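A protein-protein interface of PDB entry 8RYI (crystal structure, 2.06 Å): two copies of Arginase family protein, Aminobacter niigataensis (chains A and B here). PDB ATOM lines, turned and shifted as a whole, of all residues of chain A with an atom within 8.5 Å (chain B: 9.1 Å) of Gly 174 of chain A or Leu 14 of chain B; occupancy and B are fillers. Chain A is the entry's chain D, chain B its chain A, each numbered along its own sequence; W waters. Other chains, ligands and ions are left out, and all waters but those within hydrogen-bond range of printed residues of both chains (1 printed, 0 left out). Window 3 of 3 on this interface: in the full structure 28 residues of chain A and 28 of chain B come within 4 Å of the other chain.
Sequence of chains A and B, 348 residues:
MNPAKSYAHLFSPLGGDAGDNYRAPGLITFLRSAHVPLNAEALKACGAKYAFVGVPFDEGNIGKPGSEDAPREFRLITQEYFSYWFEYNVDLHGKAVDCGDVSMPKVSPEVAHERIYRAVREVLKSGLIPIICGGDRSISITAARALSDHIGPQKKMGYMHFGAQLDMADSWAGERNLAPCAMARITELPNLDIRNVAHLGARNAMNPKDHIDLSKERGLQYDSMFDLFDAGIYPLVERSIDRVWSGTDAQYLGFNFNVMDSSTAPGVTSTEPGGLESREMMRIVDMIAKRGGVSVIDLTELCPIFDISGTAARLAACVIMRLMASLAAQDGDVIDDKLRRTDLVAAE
Water W1 lies within hydrogen-bond range of N of Gly 174 of chain A (2.6 Å), OG of Ser 171 of chain A (2.8 Å) and NH2 of Arg 341 of chain B (3.0 Å).
No position is printed for both chains.
Of the 9 pairs that touch across the chains among the printed residues, none has its exchanged pair printed and touching as well.
Among the printed residues, merely in contact across the chains: Ser 171 of chain A with Ser 12 of chain B, Ser 171 of chain A with Arg 341 of chain B, Trp 172 of chain A with Ser 12 of chain B, Trp 172 of chain A with Pro 13 of chain B, Trp 172 of chain A with Phe 82 of chain B, Ala 173 of chain A with Leu 14 of chain B, Ala 173 of chain A with Gly 15 of chain B and Gly 174 of chain A with Leu 14 of chain B.
Gly 174 of chain A touches one residue of chain B.
Of the printed residues of chain A, Leu 14 of chain B touches Ala 173 and Gly 174.
Ala 173 of chain A touches just these residues of chain B: Pro 13 (2.7 Å), Leu 14 (3.8 Å) and Gly 15 (3.8 Å).
Of the printed residues of chain B, Ser 171 of chain A touches Ser 12 (3.5 Å) and Arg 341 (3.5 Å).
Of the printed residues of chain A, Arg 341 of chain B touches Ser 171.
Of the printed residues of chain A, Phe 82 of chain B touches Trp 172.
Of the printed residues of chain A, Ser 12 of chain B touches Ser 171 (3.5 Å) and Trp 172 (3.6 Å).
Of the printed residues of chain B, Trp 172 of chain A touches Ser 12 (3.6 Å), Pro 13 (3.4 Å) and Phe 82 (3.6 Å).
Leu 178 of chain A touches none of the printed residues of chain B.
The nearest residue of chain B that does not touch Gly 174 of chain A is Pro 13 of chain B (4.4 Å).
The nearest residue of chain A that does not touch Leu 14 of chain B is Trp 172 of chain A (5.6 Å).
The nearest printed residue of chain B that does not touch Trp 172 of chain A is Arg 341 of chain B (4.9 Å).
The guanidinium group of Arg 341 of chain B is in hydrogen-bond range of the backbone carbonyl oxygen of Ser 12 of chain B, 3.1 Å away.
O of Pro 13 of chain B sits at hydrogen-bond distance from NH2 of Arg 341 of chain B, at 3.4 Å.
The backbone NH (N) of Ala 173 of chain A sits at hydrogen-bond distance from the backbone carbonyl oxygen (O) of Pro 13 of chain B, at 2.7 Å.
Of the 11 printed residues of chain B, 6 touch a printed residue of chain A.
Along chain B the printed residues that touch a printed residue of chain A span positions 12 to 341.
Printed residues of chain A that touch a printed residue of chain B: Ser 171, Trp 172, Ala 173 and Gly 174.
Hydrophobic or aromatic side chains of chain A within 4 Å of the printed part of chain B: Trp 172.
Among the printed residues, 9 pairs touch across the chains.
Among the printed residues, no Asp or Glu carboxylate lies within 4 Å of a Lys or Arg side-chain nitrogen of the other chain.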
ATOM      1  N   ASP A 170       2.098  14.125   9.344  1.00  0.00           N
ATOM      2  CA  ASP A 170       2.097  15.586   9.367  1.00  0.00           C
ATOM      3  C   ASP A 170       3.392  16.105   9.972  1.00  0.00           C
ATOM      4  O   ASP A 170       3.989  17.059   9.458  1.00  0.00           O
ATOM      5  CB  ASP A 170       0.889  16.130  10.136  1.00  0.00           C
ATOM      6  CG  ASP A 170       0.735  17.652   9.993  1.00  0.00           C
ATOM      7  OD1 ASP A 170       1.056  18.194   8.912  1.00  0.00           O
ATOM      8  OD2 ASP A 170       0.281  18.313  10.958  1.00  0.00           O
ATOM      9  N   SER A 171       3.855  15.470  11.046  1.00  0.00           N
ATOM     10  CA  SER A 171       5.186  15.732  11.563  1.00  0.00           C
ATOM     11  C   SER A 171       5.733  14.449  12.164  1.00  0.00           C
ATOM     12  O   SER A 171       4.984  13.545  12.544  1.00  0.00           O
ATOM     13  CB  SER A 171       5.199  16.856  12.603  1.00  0.00           C
ATOM     14  OG  SER A 171       4.618  16.433  13.821  1.00  0.00           O
ATOM     15  N   TRP A 172       7.060  14.387  12.247  1.00  0.00           N
ATOM     16  CA  TRP A 172       7.770  13.216  12.743  1.00  0.00           C
ATOM     17  C   TRP A 172       8.952  13.704  13.564  1.00  0.00           C
ATOM     18  O   TRP A 172       9.784  14.462  13.057  1.00  0.00           O
ATOM     19  CB  TRP A 172       8.233  12.330  11.577  1.00  0.00           C
ATOM     20  CG  TRP A 172       8.872  11.031  11.968  1.00  0.00           C
ATOM     21  CD1 TRP A 172      10.130  10.844  12.461  1.00  0.00           C
ATOM     22  CD2 TRP A 172       8.277   9.733  11.886  1.00  0.00           C
ATOM     23  NE1 TRP A 172      10.354   9.509  12.692  1.00  0.00           N
ATOM     24  CE2 TRP A 172       9.232   8.805  12.350  1.00  0.00           C
ATOM     25  CE3 TRP A 172       7.026   9.263  11.469  1.00  0.00           C
ATOM     26  CZ2 TRP A 172       8.980   7.438  12.401  1.00  0.00           C
ATOM     27  CZ3 TRP A 172       6.775   7.902  11.525  1.00  0.00           C
ATOM     28  CH2 TRP A 172       7.749   7.005  11.988  1.00  0.00           C
ATOM     29  N   ALA A 173       9.003  13.311  14.837  1.00  0.00           N
ATOM     30  CA  ALA A 173      10.054  13.755  15.751  1.00  0.00           C
ATOM     31  C   ALA A 173      10.208  15.275  15.757  1.00  0.00           C
ATOM     32  O   ALA A 173      11.315  15.798  15.907  1.00  0.00           O
ATOM     33  CB  ALA A 173      11.388  13.083  15.420  1.00  0.00           C
ATOM     34  N   GLY A 174       9.102  15.999  15.586  1.00  0.00           N
ATOM     35  CA  GLY A 174       9.134  17.447  15.551  1.00  0.00           C
ATOM     36  C   GLY A 174       9.533  18.069  14.226  1.00  0.00           C
ATOM     37  O   GLY A 174       9.537  19.304  14.120  1.00  0.00           O
ATOM     38  N   GLU A 175       9.872  17.264  13.224  1.00  0.00           N
ATOM     39  CA  GLU A 175      10.256  17.738  11.904  1.00  0.00           C
ATOM     40  C   GLU A 175       9.060  17.618  10.960  1.00  0.00           C
ATOM     41  O   GLU A 175       8.155  16.810  11.175  1.00  0.00           O
ATOM     42  CB  GLU A 175      11.428  16.911  11.366  1.00  0.00           C
ATOM     43  CG  GLU A 175      12.698  16.896  12.222  1.00  0.00           C
ATOM     44  CD  GLU A 175      13.514  18.163  12.109  1.00  0.00           C
ATOM     45  OE1 GLU A 175      13.787  18.591  10.972  1.00  0.00           O
ATOM     46  OE2 GLU A 175      13.914  18.717  13.152  1.00  0.00           O
ATOM     47  N   ARG A 176       9.063  18.418   9.894  1.00  0.00           N
ATOM     48  CA  ARG A 176       7.981  18.357   8.922  1.00  0.00           C
ATOM     49  C   ARG A 176       8.425  17.913   7.532  1.00  0.00           C
ATOM     50  O   ARG A 176       7.568  17.748   6.654  1.00  0.00           O
ATOM     51  CB  ARG A 176       7.263  19.713   8.837  1.00  0.00           C
ATOM     52  CG  ARG A 176       6.594  20.120  10.148  1.00  0.00           C
ATOM     53  CD  ARG A 176       5.743  21.378  10.010  1.00  0.00           C
ATOM     54  NE  ARG A 176       4.514  21.152   9.254  1.00  0.00           N
ATOM     55  CZ  ARG A 176       3.366  20.755   9.787  1.00  0.00           C
ATOM     56  NH1 ARG A 176       3.258  20.494  11.079  1.00  0.00           N
ATOM     57  NH2 ARG A 176       2.300  20.617   9.006  1.00  0.00           N
ATOM     58  N   ASN A 177       9.724  17.679   7.307  1.00  0.00           N
ATOM     59  CA  ASN A 177      10.177  17.333   5.966  1.00  0.00           C
ATOM     60  C   ASN A 177      11.102  16.119   5.959  1.00  0.00           C
ATOM     61  O   ASN A 177      11.936  15.977   5.057  1.00  0.00           O
ATOM     62  CB  ASN A 177      10.864  18.531   5.311  1.00  0.00           C
ATOM     63  CG  ASN A 177       9.893  19.665   4.991  1.00  0.00           C
ATOM     64  OD1 ASN A 177       9.060  19.561   4.086  1.00  0.00           O
ATOM     65  ND2 ASN A 177       9.980  20.748   5.761  1.00  0.00           N
ATOM     66  N   LEU A 178      10.947  15.213   6.923  1.00  0.00           N
ATOM     67  CA  LEU A 178      11.671  13.953   6.852  1.00  0.00           C
ATOM     68  C   LEU A 178      10.924  12.987   5.939  1.00  0.00           C
ATOM     69  O   LEU A 178       9.782  13.233   5.547  1.00  0.00           O
ATOM     70  CB  LEU A 178      11.870  13.354   8.242  1.00  0.00           C
ATOM     71  CG  LEU A 178      12.676  14.246   9.189  1.00  0.00           C
ATOM     72  CD1 LEU A 178      12.795  13.628  10.579  1.00  0.00           C
ATOM     73  CD2 LEU A 178      14.048  14.538   8.593  1.00  0.00           C
ATOM     74  N   CYS A 181       7.300  12.129   6.168  1.00  0.00           N
ATOM     75  CA  CYS A 181       6.404  13.265   5.992  1.00  0.00           C
ATOM     76  C   CYS A 181       6.097  13.564   4.524  1.00  0.00           C
ATOM     77  O   CYS A 181       5.332  14.498   4.243  1.00  0.00           O
ATOM     78  CB  CYS A 181       7.011  14.507   6.643  1.00  0.00           C
ATOM     79  SG  CYS A 181       7.544  14.289   8.365  1.00  0.00           S
ATOM     80  N   TYR B   7      -0.829   5.497  24.495  1.00  0.00           N
ATOM     81  CA  TYR B   7      -1.110   5.107  23.117  1.00  0.00           C
ATOM     82  C   TYR B   7      -0.204   5.790  22.099  1.00  0.00           C
ATOM     83  O   TYR B   7      -0.473   5.709  20.899  1.00  0.00           O
ATOM     84  CB  TYR B   7      -2.578   5.355  22.765  1.00  0.00           C
ATOM     85  CG  TYR B   7      -3.523   4.276  23.251  1.00  0.00           C
ATOM     86  CD1 TYR B   7      -3.263   2.932  22.977  1.00  0.00           C
ATOM     87  CD2 TYR B   7      -4.682   4.593  23.955  1.00  0.00           C
ATOM     88  CE1 TYR B   7      -4.126   1.931  23.397  1.00  0.00           C
ATOM     89  CE2 TYR B   7      -5.550   3.599  24.384  1.00  0.00           C
ATOM     90  CZ  TYR B   7      -5.268   2.272  24.103  1.00  0.00           C
ATOM     91  OH  TYR B   7      -6.132   1.284  24.530  1.00  0.00           O
ATOM     92  N   ALA B   8       0.845   6.481  22.553  1.00  0.00           N
ATOM     93  CA  ALA B   8       1.726   7.213  21.648  1.00  0.00           C
ATOM     94  C   ALA B   8       2.380   6.309  20.616  1.00  0.00           C
ATOM     95  O   ALA B   8       2.676   6.758  19.503  1.00  0.00           O
ATOM     96  CB  ALA B   8       2.809   7.941  22.446  1.00  0.00           C
ATOM     97  N   HIS B   9       2.595   5.036  20.949  1.00  0.00           N
ATOM     98  CA  HIS B   9       3.229   4.110  20.022  1.00  0.00           C
ATOM     99  C   HIS B   9       2.361   3.806  18.810  1.00  0.00           C
ATOM    100  O   HIS B   9       2.835   3.135  17.891  1.00  0.00           O
ATOM    101  CB  HIS B   9       3.583   2.816  20.743  1.00  0.00           C
ATOM    102  CG  HIS B   9       2.387   2.067  21.231  1.00  0.00           C
ATOM    103  ND1 HIS B   9       1.779   2.345  22.433  1.00  0.00           N
ATOM    104  CD2 HIS B   9       1.673   1.064  20.670  1.00  0.00           C
ATOM    105  CE1 HIS B   9       0.746   1.539  22.598  1.00  0.00           C
ATOM    106  NE2 HIS B   9       0.662   0.751  21.543  1.00  0.00           N
ATOM    107  N   PHE B  11       1.265   6.175  16.859  1.00  0.00           N
ATOM    108  CA  PHE B  11       1.378   7.346  16.010  1.00  0.00           C
ATOM    109  C   PHE B  11       2.839   7.686  15.751  1.00  0.00           C
ATOM    110  O   PHE B  11       3.757   7.097  16.334  1.00  0.00           O
ATOM    111  CB  PHE B  11       0.655   8.529  16.642  1.00  0.00           C
ATOM    112  CG  PHE B  11      -0.756   8.223  17.004  1.00  0.00           C
ATOM    113  CD1 PHE B  11      -1.743   8.194  16.031  1.00  0.00           C
ATOM    114  CD2 PHE B  11      -1.099   7.941  18.318  1.00  0.00           C
ATOM    115  CE1 PHE B  11      -3.048   7.900  16.362  1.00  0.00           C
ATOM    116  CE2 PHE B  11      -2.403   7.651  18.664  1.00  0.00           C
ATOM    117  CZ  PHE B  11      -3.383   7.631  17.689  1.00  0.00           C
ATOM    118  N   SER B  12       3.033   8.633  14.837  1.00  0.00           N
ATOM    119  CA  SER B  12       4.357   9.157  14.544  1.00  0.00           C
ATOM    120  C   SER B  12       5.021   9.667  15.824  1.00  0.00           C
ATOM    121  O   SER B  12       4.368  10.328  16.640  1.00  0.00           O
ATOM    122  CB  SER B  12       4.256  10.284  13.509  1.00  0.00           C
ATOM    123  OG  SER B  12       3.617   9.837  12.326  1.00  0.00           O
ATOM    124  N   PRO B  13       6.309   9.384  16.025  1.00  0.00           N
ATOM    125  CA  PRO B  13       6.987   9.805  17.259  1.00  0.00           C
ATOM    126  C   PRO B  13       7.031  11.320  17.412  1.00  0.00           C
ATOM    127  O   PRO B  13       7.227  12.056  16.443  1.00  0.00           O
ATOM    128  CB  PRO B  13       8.398   9.220  17.110  1.00  0.00           C
ATOM    129  CG  PRO B  13       8.342   8.290  15.927  1.00  0.00           C
ATOM    130  CD  PRO B  13       7.222   8.742  15.068  1.00  0.00           C
ATOM    131  N   LEU B  14       6.847  11.781  18.650  1.00  0.00           N
ATOM    132  CA  LEU B  14       6.947  13.202  18.961  1.00  0.00           C
ATOM    133  C   LEU B  14       8.377  13.697  19.156  1.00  0.00           C
ATOM    134  O   LEU B  14       8.586  14.919  19.180  1.00  0.00           O
ATOM    135  CB  LEU B  14       6.129  13.527  20.212  1.00  0.00           C
ATOM    136  CG  LEU B  14       4.613  13.392  20.123  1.00  0.00           C
ATOM    137  CD1 LEU B  14       4.032  13.333  21.521  1.00  0.00           C
ATOM    138  CD2 LEU B  14       4.045  14.578  19.362  1.00  0.00           C
ATOM    139  N   GLY B  15       9.352  12.804  19.325  1.00  0.00           N
ATOM    140  CA  GLY B  15      10.741  13.213  19.482  1.00  0.00           C
ATOM    141  C   GLY B  15      11.136  13.638  20.893  1.00  0.00           C
ATOM    142  O   GLY B  15      11.075  14.820  21.264  1.00  0.00           O
ATOM    143  N   PHE B  82       6.785  -1.436  13.877  1.00  0.00           N
ATOM    144  CA  PHE B  82       5.780  -0.800  14.706  1.00  0.00           C
ATOM    145  C   PHE B  82       4.764  -1.841  15.151  1.00  0.00           C
ATOM    146  O   PHE B  82       4.624  -2.910  14.545  1.00  0.00           O
ATOM    147  CB  PHE B  82       5.072   0.319  13.948  1.00  0.00           C
ATOM    148  CG  PHE B  82       5.829   1.602  13.918  1.00  0.00           C
ATOM    149  CD1 PHE B  82       6.939   1.750  13.106  1.00  0.00           C
ATOM    150  CD2 PHE B  82       5.440   2.657  14.731  1.00  0.00           C
ATOM    151  CE1 PHE B  82       7.641   2.931  13.082  1.00  0.00           C
ATOM    152  CE2 PHE B  82       6.137   3.847  14.725  1.00  0.00           C
ATOM    153  CZ  PHE B  82       7.250   3.980  13.888  1.00  0.00           C
ATOM    154  N   ARG B 341      -3.678  11.537  17.321  1.00  0.00           N
ATOM    155  CA  ARG B 341      -2.346  11.820  17.843  1.00  0.00           C
ATOM    156  C   ARG B 341      -2.414  12.927  18.895  1.00  0.00           C
ATOM    157  O   ARG B 341      -2.636  14.097  18.567  1.00  0.00           O
ATOM    158  CB  ARG B 341      -1.417  12.183  16.680  1.00  0.00           C
ATOM    159  CG  ARG B 341       0.052  12.335  17.017  1.00  0.00           C
ATOM    160  CD  ARG B 341       0.852  12.358  15.724  1.00  0.00           C
ATOM    161  NE  ARG B 341       2.285  12.507  15.943  1.00  0.00           N
ATOM    162  CZ  ARG B 341       2.915  13.675  15.975  1.00  0.00           C
ATOM    163  NH1 ARG B 341       2.260  14.816  15.841  1.00  0.00           N
ATOM    164  NH2 ARG B 341       4.236  13.696  16.140  1.00  0.00           N
ATOM    165  N   THR B 342      -2.244  12.550  20.164  1.00  0.00           N
ATOM    166  CA  THR B 342      -2.486  13.431  21.314  1.00  0.00           C
ATOM    167  C   THR B 342      -1.456  13.194  22.424  1.00  0.00           C
ATOM    168  O   THR B 342      -0.971  14.135  23.063  1.00  0.00           O
ATOM    169  CB  THR B 342      -3.918  13.221  21.892  1.00  0.00           C
ATOM    170  OG1 THR B 342      -4.859  14.025  21.171  1.00  0.00           O
ATOM    171  CG2 THR B 342      -3.982  13.578  23.367  1.00  0.00           C
HETATM  172  O   HOH W   1       6.496  15.667  15.803  1.00  0.00           O
